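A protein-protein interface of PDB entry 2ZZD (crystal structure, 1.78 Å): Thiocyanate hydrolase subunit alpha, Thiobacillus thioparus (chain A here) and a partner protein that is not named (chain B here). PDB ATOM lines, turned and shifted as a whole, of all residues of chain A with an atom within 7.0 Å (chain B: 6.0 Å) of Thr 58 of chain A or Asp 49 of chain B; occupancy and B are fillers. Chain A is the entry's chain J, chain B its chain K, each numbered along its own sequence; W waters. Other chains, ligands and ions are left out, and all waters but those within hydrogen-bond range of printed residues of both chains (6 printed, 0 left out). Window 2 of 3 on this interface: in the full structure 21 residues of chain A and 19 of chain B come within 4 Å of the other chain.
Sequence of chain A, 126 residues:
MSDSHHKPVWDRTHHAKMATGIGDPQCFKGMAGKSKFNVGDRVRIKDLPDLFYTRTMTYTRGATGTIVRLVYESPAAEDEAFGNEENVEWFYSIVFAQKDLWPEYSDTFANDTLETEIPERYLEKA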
ATOM      1  N   ASP A  47     -24.489  23.161 -14.411  1.00  0.00           N
ATOM      2  CA  ASP A  47     -23.377  23.365 -13.490  1.00  0.00           C
ATOM      3  C   ASP A  47     -23.696  24.535 -12.570  1.00  0.00           C
ATOM      4  O   ASP A  47     -23.128  25.620 -12.697  1.00  0.00           O
ATOM      5  CB  ASP A  47     -22.083  23.624 -14.268  1.00  0.00           C
ATOM      6  CG  ASP A  47     -20.855  23.614 -13.375  1.00  0.00           C
ATOM      7  OD1 ASP A  47     -20.934  23.071 -12.251  1.00  0.00           O
ATOM      8  OD2 ASP A  47     -19.809  24.147 -13.801  1.00  0.00           O
ATOM      9  N   ASP A  50     -21.679  25.714  -6.535  1.00  0.00           N
ATOM     10  CA  ASP A  50     -21.627  24.708  -5.479  1.00  0.00           C
ATOM     11  C   ASP A  50     -21.055  25.213  -4.156  1.00  0.00           C
ATOM     12  O   ASP A  50     -20.699  24.421  -3.280  1.00  0.00           O
ATOM     13  CB  ASP A  50     -20.830  23.485  -5.957  1.00  0.00           C
ATOM     14  CG  ASP A  50     -19.388  23.815  -6.296  1.00  0.00           C
ATOM     15  OD1 ASP A  50     -19.045  25.013  -6.368  1.00  0.00           O
ATOM     16  OD2 ASP A  50     -18.597  22.869  -6.497  1.00  0.00           O
ATOM     17  N   THR A  54     -23.379  20.892  -1.816  1.00  0.00           N
ATOM     18  CA  THR A  54     -24.036  20.306  -2.971  1.00  0.00           C
ATOM     19  C   THR A  54     -23.906  18.797  -2.877  1.00  0.00           C
ATOM     20  O   THR A  54     -22.954  18.279  -2.293  1.00  0.00           O
ATOM     21  CB  THR A  54     -23.417  20.740  -4.320  1.00  0.00           C
ATOM     22  OG1 THR A  54     -24.226  20.228  -5.390  1.00  0.00           O
ATOM     23  CG2 THR A  54     -22.001  20.185  -4.483  1.00  0.00           C
ATOM     24  N   ARG A  55     -24.888  18.094  -3.422  1.00  0.00           N
ATOM     25  CA  ARG A  55     -24.839  16.649  -3.444  1.00  0.00           C
ATOM     26  C   ARG A  55     -24.952  16.187  -4.895  1.00  0.00           C
ATOM     27  O   ARG A  55     -25.276  15.036  -5.178  1.00  0.00           O
ATOM     28  CB  ARG A  55     -25.935  16.045  -2.559  1.00  0.00           C
ATOM     29  CG  ARG A  55     -25.691  16.299  -1.066  1.00  0.00           C
ATOM     30  CD  ARG A  55     -26.514  15.364  -0.172  1.00  0.00           C
ATOM     31  NE  ARG A  55     -26.006  13.990  -0.154  1.00  0.00           N
ATOM     32  CZ  ARG A  55     -24.936  13.592   0.537  1.00  0.00           C
ATOM     33  NH1 ARG A  55     -24.247  14.459   1.278  1.00  0.00           N
ATOM     34  NH2 ARG A  55     -24.547  12.321   0.491  1.00  0.00           N
ATOM     35  N   THR A  56     -24.701  17.116  -5.819  1.00  0.00           N
ATOM     36  CA  THR A  56     -24.708  16.797  -7.247  1.00  0.00           C
ATOM     37  C   THR A  56     -23.226  16.852  -7.617  1.00  0.00           C
ATOM     38  O   THR A  56     -22.664  17.923  -7.865  1.00  0.00           O
ATOM     39  CB  THR A  56     -25.520  17.812  -8.077  1.00  0.00           C
ATOM     40  OG1 THR A  56     -26.892  17.771  -7.664  1.00  0.00           O
ATOM     41  CG2 THR A  56     -25.449  17.460  -9.566  1.00  0.00           C
ATOM     42  N   MET A  57     -22.605  15.674  -7.618  1.00  0.00           N
ATOM     43  CA  MET A  57     -21.180  15.513  -7.883  1.00  0.00           C
ATOM     44  C   MET A  57     -20.637  16.287  -9.070  1.00  0.00           C
ATOM     45  O   MET A  57     -21.264  16.357 -10.124  1.00  0.00           O
ATOM     46  CB  MET A  57     -20.843  14.031  -8.061  1.00  0.00           C
ATOM     47  CG  MET A  57     -21.123  13.163  -6.829  1.00  0.00           C
ATOM     48  SD  MET A  57     -22.884  12.811  -6.565  1.00  0.00           S
ATOM     49  CE  MET A  57     -23.239  11.850  -8.032  1.00  0.00           C
ATOM     50  N   THR A  58     -19.453  16.864  -8.883  1.00  0.00           N
ATOM     51  CA  THR A  58     -18.801  17.622  -9.937  1.00  0.00           C
ATOM     52  C   THR A  58     -18.611  16.762 -11.186  1.00  0.00           C
ATOM     53  O   THR A  58     -18.749  17.260 -12.304  1.00  0.00           O
ATOM     54  CB  THR A  58     -17.423  18.153  -9.472  1.00  0.00           C
ATOM     55  OG1 THR A  58     -17.604  19.041  -8.364  1.00  0.00           O
ATOM     56  CG2 THR A  58     -16.731  18.909 -10.603  1.00  0.00           C
ATOM     57  N   TYR A  59     -18.331  15.469 -11.015  1.00  0.00           N
ATOM     58  CA  TYR A  59     -18.115  14.623 -12.187  1.00  0.00           C
ATOM     59  C   TYR A  59     -19.315  14.509 -13.128  1.00  0.00           C
ATOM     60  O   TYR A  59     -19.156  14.083 -14.275  1.00  0.00           O
ATOM     61  CB  TYR A  59     -17.589  13.231 -11.772  1.00  0.00           C
ATOM     62  CG  TYR A  59     -18.586  12.268 -11.158  1.00  0.00           C
ATOM     63  CD1 TYR A  59     -19.539  11.620 -11.945  1.00  0.00           C
ATOM     64  CD2 TYR A  59     -18.532  11.954  -9.799  1.00  0.00           C
ATOM     65  CE1 TYR A  59     -20.412  10.672 -11.393  1.00  0.00           C
ATOM     66  CE2 TYR A  59     -19.399  11.009  -9.236  1.00  0.00           C
ATOM     67  CZ  TYR A  59     -20.334  10.371 -10.040  1.00  0.00           C
ATOM     68  OH  TYR A  59     -21.175   9.428  -9.491  1.00  0.00           O
ATOM     69  N   THR A  60     -20.503  14.900 -12.668  1.00  0.00           N
ATOM     70  CA  THR A  60     -21.694  14.840 -13.523  1.00  0.00           C
ATOM     71  C   THR A  60     -22.022  16.153 -14.244  1.00  0.00           C
ATOM     72  O   THR A  60     -22.828  16.160 -15.183  1.00  0.00           O
ATOM     73  CB  THR A  60     -22.981  14.491 -12.733  1.00  0.00           C
ATOM     74  OG1 THR A  60     -23.283  15.562 -11.825  1.00  0.00           O
ATOM     75  CG2 THR A  60     -22.818  13.187 -11.967  1.00  0.00           C
ATOM     76  N   ARG A  61     -21.413  17.256 -13.816  1.00  0.00           N
ATOM     77  CA  ARG A  61     -21.723  18.559 -14.404  1.00  0.00           C
ATOM     78  C   ARG A  61     -21.515  18.649 -15.915  1.00  0.00           C
ATOM     79  O   ARG A  61     -20.439  18.342 -16.429  1.00  0.00           O
ATOM     80  CB  ARG A  61     -20.919  19.671 -13.709  1.00  0.00           C
ATOM     81  CG  ARG A  61     -21.014  19.691 -12.172  1.00  0.00           C
ATOM     82  CD  ARG A  61     -22.446  19.538 -11.672  1.00  0.00           C
ATOM     83  NE  ARG A  61     -22.562  19.633 -10.215  1.00  0.00           N
ATOM     84  CZ  ARG A  61     -22.719  20.773  -9.542  1.00  0.00           C
ATOM     85  NH1 ARG A  61     -22.770  21.931 -10.189  1.00  0.00           N
ATOM     86  NH2 ARG A  61     -22.854  20.757  -8.221  1.00  0.00           N
ATOM     87  N   GLY A  62     -22.566  19.069 -16.617  1.00  0.00           N
ATOM     88  CA  GLY A  62     -22.489  19.229 -18.060  1.00  0.00           C
ATOM     89  C   GLY A  62     -22.692  17.959 -18.862  1.00  0.00           C
ATOM     90  O   GLY A  62     -22.708  17.996 -20.093  1.00  0.00           O
ATOM     91  N   ARG B  41     -12.392  27.765  -7.782  1.00  0.00           N
ATOM     92  CA  ARG B  41     -13.308  26.631  -7.756  1.00  0.00           C
ATOM     93  C   ARG B  41     -12.740  25.482  -6.920  1.00  0.00           C
ATOM     94  O   ARG B  41     -13.472  24.813  -6.188  1.00  0.00           O
ATOM     95  CB  ARG B  41     -13.607  26.135  -9.178  1.00  0.00           C
ATOM     96  CG  ARG B  41     -14.671  25.038  -9.204  1.00  0.00           C
ATOM     97  CD  ARG B  41     -15.030  24.556 -10.608  1.00  0.00           C
ATOM     98  NE  ARG B  41     -16.081  23.544 -10.530  1.00  0.00           N
ATOM     99  CZ  ARG B  41     -17.124  23.468 -11.353  1.00  0.00           C
ATOM    100  NH1 ARG B  41     -17.266  24.345 -12.338  1.00  0.00           N
ATOM    101  NH2 ARG B  41     -18.047  22.529 -11.171  1.00  0.00           N
ATOM    102  N   ARG B  45     -14.403  24.279  -3.258  1.00  0.00           N
ATOM    103  CA  ARG B  45     -15.005  22.967  -3.496  1.00  0.00           C
ATOM    104  C   ARG B  45     -15.600  22.454  -2.191  1.00  0.00           C
ATOM    105  O   ARG B  45     -15.215  22.905  -1.115  1.00  0.00           O
ATOM    106  CB  ARG B  45     -13.913  21.962  -3.869  1.00  0.00           C
ATOM    107  CG  ARG B  45     -13.020  21.656  -2.645  1.00  0.00           C
ATOM    108  CD  ARG B  45     -12.066  20.486  -2.830  1.00  0.00           C
ATOM    109  NE  ARG B  45     -12.715  19.313  -3.405  1.00  0.00           N
ATOM    110  CZ  ARG B  45     -12.139  18.123  -3.530  1.00  0.00           C
ATOM    111  NH1 ARG B  45     -10.894  17.934  -3.107  1.00  0.00           N
ATOM    112  NH2 ARG B  45     -12.795  17.131  -4.107  1.00  0.00           N
ATOM    113  N   VAL B  46     -16.525  21.504  -2.287  1.00  0.00           N
ATOM    114  CA  VAL B  46     -17.074  20.873  -1.094  1.00  0.00           C
ATOM    115  C   VAL B  46     -16.157  19.634  -1.012  1.00  0.00           C
ATOM    116  O   VAL B  46     -16.165  18.797  -1.910  1.00  0.00           O
ATOM    117  CB  VAL B  46     -18.572  20.464  -1.288  1.00  0.00           C
ATOM    118  CG1 VAL B  46     -19.433  21.719  -1.459  1.00  0.00           C
ATOM    119  CG2 VAL B  46     -18.725  19.551  -2.511  1.00  0.00           C
ATOM    120  N   PRO B  47     -15.341  19.520   0.054  1.00  0.00           N
ATOM    121  CA  PRO B  47     -14.401  18.408   0.253  1.00  0.00           C
ATOM    122  C   PRO B  47     -14.871  16.979   0.007  1.00  0.00           C
ATOM    123  O   PRO B  47     -14.089  16.143  -0.441  1.00  0.00           O
ATOM    124  CB  PRO B  47     -13.941  18.592   1.698  1.00  0.00           C
ATOM    125  CG  PRO B  47     -14.063  20.053   1.912  1.00  0.00           C
ATOM    126  CD  PRO B  47     -15.380  20.376   1.254  1.00  0.00           C
ATOM    127  N   HIS B  48     -16.135  16.694   0.306  1.00  0.00           N
ATOM    128  CA  HIS B  48     -16.642  15.335   0.158  1.00  0.00           C
ATOM    129  C   HIS B  48     -16.829  14.839  -1.273  1.00  0.00           C
ATOM    130  O   HIS B  48     -16.985  13.640  -1.499  1.00  0.00           O
ATOM    131  CB  HIS B  48     -17.952  15.169   0.956  1.00  0.00           C
ATOM    132  CG  HIS B  48     -19.142  15.866   0.362  1.00  0.00           C
ATOM    133  ND1 HIS B  48     -20.420  15.678   0.846  1.00  0.00           N
ATOM    134  CD2 HIS B  48     -19.257  16.736  -0.670  1.00  0.00           C
ATOM    135  CE1 HIS B  48     -21.271  16.399   0.137  1.00  0.00           C
ATOM    136  NE2 HIS B  48     -20.592  17.051  -0.790  1.00  0.00           N
ATOM    137  N   ASP B  49     -16.775  15.756  -2.236  1.00  0.00           N
ATOM    138  CA  ASP B  49     -16.978  15.429  -3.648  1.00  0.00           C
ATOM    139  C   ASP B  49     -15.681  14.955  -4.318  1.00  0.00           C
ATOM    140  O   ASP B  49     -15.049  15.706  -5.060  1.00  0.00           O
ATOM    141  CB  ASP B  49     -17.535  16.677  -4.343  1.00  0.00           C
ATOM    142  CG  ASP B  49     -18.039  16.402  -5.743  1.00  0.00           C
ATOM    143  OD1 ASP B  49     -18.076  15.221  -6.157  1.00  0.00           O
ATOM    144  OD2 ASP B  49     -18.410  17.377  -6.429  1.00  0.00           O
ATOM    145  N   VAL B  50     -15.315  13.696  -4.077  1.00  0.00           N
ATOM    146  CA  VAL B  50     -14.069  13.128  -4.606  1.00  0.00           C
ATOM    147  C   VAL B  50     -14.192  12.153  -5.784  1.00  0.00           C
ATOM    148  O   VAL B  50     -13.180  11.735  -6.351  1.00  0.00           O
ATOM    149  CB  VAL B  50     -13.293  12.397  -3.481  1.00  0.00           C
ATOM    150  CG1 VAL B  50     -13.083  13.336  -2.305  1.00  0.00           C
ATOM    151  CG2 VAL B  50     -14.059  11.159  -3.031  1.00  0.00           C
ATOM    152  N   GLY B  51     -15.417  11.783  -6.145  1.00  0.00           N
ATOM    153  CA  GLY B  51     -15.601  10.848  -7.244  1.00  0.00           C
ATOM    154  C   GLY B  51     -14.890  11.262  -8.525  1.00  0.00           C
ATOM    155  O   GLY B  51     -15.048  12.390  -8.990  1.00  0.00           O
ATOM    156  N   GLU B  53     -11.588  11.420  -8.925  1.00  0.00           N
ATOM    157  CA  GLU B  53     -10.219  11.841  -8.646  1.00  0.00           C
ATOM    158  C   GLU B  53      -9.285  10.642  -8.788  1.00  0.00           C
ATOM    159  O   GLU B  53      -9.598   9.539  -8.346  1.00  0.00           O
ATOM    160  CB  GLU B  53     -10.110  12.413  -7.230  1.00  0.00           C
ATOM    161  CG  GLU B  53     -10.714  13.805  -7.073  1.00  0.00           C
ATOM    162  CD  GLU B  53     -10.691  14.296  -5.638  1.00  0.00           C
ATOM    163  OE1 GLU B  53      -9.890  13.766  -4.840  1.00  0.00           O
ATOM    164  OE2 GLU B  53     -11.461  15.224  -5.307  1.00  0.00           O
ATOM    165  N   TYR B 103     -10.582  16.976   6.681  1.00  0.00           N
ATOM    166  CA  TYR B 103     -11.369  15.995   5.952  1.00  0.00           C
ATOM    167  C   TYR B 103     -10.575  14.744   5.586  1.00  0.00           C
ATOM    168  O   TYR B 103     -11.102  13.631   5.645  1.00  0.00           O
ATOM    169  CB  TYR B 103     -11.961  16.611   4.681  1.00  0.00           C
ATOM    170  CG  TYR B 103     -12.902  15.662   3.980  1.00  0.00           C
ATOM    171  CD1 TYR B 103     -14.088  15.255   4.593  1.00  0.00           C
ATOM    172  CD2 TYR B 103     -12.582  15.118   2.735  1.00  0.00           C
ATOM    173  CE1 TYR B 103     -14.928  14.329   3.987  1.00  0.00           C
ATOM    174  CE2 TYR B 103     -13.417  14.189   2.123  1.00  0.00           C
ATOM    175  CZ  TYR B 103     -14.586  13.796   2.755  1.00  0.00           C
ATOM    176  OH  TYR B 103     -15.398  12.859   2.164  1.00  0.00           O
HETATM  177  O   HOH W   1     -19.470  21.168  -8.776  1.00  0.00           O
HETATM  178  O   HOH W   2     -17.374  20.461  -5.025  1.00  0.00           O
HETATM  179  O   HOH W   3     -16.512  21.752  -8.446  1.00  0.00           O
HETATM  180  O   HOH W   4     -18.257  25.524  -8.970  1.00  0.00           O
HETATM  181  O   HOH W   5     -21.693  13.852   2.500  1.00  0.00           O
HETATM  182  O   HOH W   6     -16.829  14.706  -8.522  1.00  0.00           O
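The side-chain carboxylate of Asp 47 of chain A lies within salt-bridge range of the guanidinium group of Arg 41 of chain B (2.9 Å).
The backbone carbonyl oxygen of Thr 54 of chain A lies within hydrogen-bond range of a ring nitrogen (NE2) of His 48 of chain B (3.1 Å).
The side-chain hydroxyl (OG1) of Thr 58 of chain A lies within hydrogen-bond range of the side-chain carboxylate (OD2) of Asp 49 of chain B (2.7 Å).
NH1 of Arg 61 of chain A lies within salt-bridge range of OD1 of Asp 47 of chain A, at 3.0 Å.
OG1 of Thr 54 of chain A sits at hydrogen-bond distance from N of Thr 56 of chain A (3.2 Å).
The side-chain hydroxyl (OG1) of Thr 54 of chain A lies within hydrogen-bond range of the guanidinium group (NH2) of Arg 61 of chain A.
OG1 of Thr 60 of chain A is in hydrogen-bond range of O of Met 57 of chain A (2.8 Å).
NH2 of Arg 45 of chain B is in hydrogen-bond range of O of Asp 49 of chain B (2.8 Å).
Among the printed residues, pairs that only touch across the chains: Asp 50 of chain A with Val 46 of chain B (3.5 Å), Thr 54 of chain A with Val 46 of chain B (3.9 Å), Arg 55 of chain A with His 48 of chain B (3.7 Å), Met 57 of chain A with Asp 49 of chain B (3.6 Å), Thr 58 of chain A with Arg 41 of chain B (3.9 Å) and Tyr 59 of chain A with Gly 51 of chain B (3.6 Å).
Printed residues of chain B within 4 Å of Asp 47 of chain A: Arg 41.
Of the printed residues of chain B, Arg 55 of chain A touches His 48.
Thr 58 of chain A touches two residues of chain B.
Of chain A, only Met 57 (3.6 Å) and Thr 58 (2.7 Å) come within 4 Å of Asp 49 of chain B.
The nearest printed residue of chain B that does not touch Thr 58 of chain A is Val 46 of chain B (6.0 Å).
The nearest residue of chain A that does not touch Asp 49 of chain B is Thr 56 of chain A (4.5 Å).
The nearest printed residue of chain B that does not touch Asp 47 of chain A is Asp 49 of chain B (8.5 Å).
Printed residues of chain A that touch a printed residue of chain B: Asp 47, Asp 50, Thr 54, Arg 55, Met 57, Thr 58 and Tyr 59.
Hydrophobic or aromatic side chains of chain A that line the printed part of chain B: Met 57 and Tyr 59.
Of the 10 printed residues of chain B, 5 touch a printed residue of chain A.
Hydrophobic or aromatic side chains of chain B within 4 Å of the printed part of chain A: Val 46 and His 48.
Among the printed residues, Asp or Glu carboxylates within 4 Å of a Lys or Arg side-chain nitrogen of the other chain: Asp 47 of chain A with Arg 41 of chain B (2.9 Å).
Water W6 lies within hydrogen-bond range of OD1 of Asp 49 of chain B (2.7 Å), O of Gly 51 of chain B (3.0 Å), N of Tyr 59 of chain A (3.0 Å) and N of Thr 58 of chain A (3.4 Å).
Water W4 lies within hydrogen-bond range of OD1 of Asp 50 of chain A (2.8 Å) and NE of Arg 41 of chain B (3.3 Å).
Water W5 lies within hydrogen-bond range of a ring nitrogen (ND1) of His 48 of chain B (2.8 Å) and the guanidinium group (NH1) of Arg 55 of chain A (2.9 Å).
Water W3 lies within hydrogen-bond range of NE of Arg 41 of chain B (2.8 Å), OG1 of Thr 58 of chain A (2.9 Å) and OD2 of Asp 50 of chain A (3.1 Å).
Water W1 lies within hydrogen-bond range of OG1 of Thr 58 of chain A, OD2 of Asp 50 of chain A, NH2 of Arg 41 of chain B and NH2 of Arg 61 of chain A.
Water W2 lies within hydrogen-bond range of N of Val 46 of chain B (3.1 Å) and OD2 of Asp 50 of chain A (3.1 Å).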
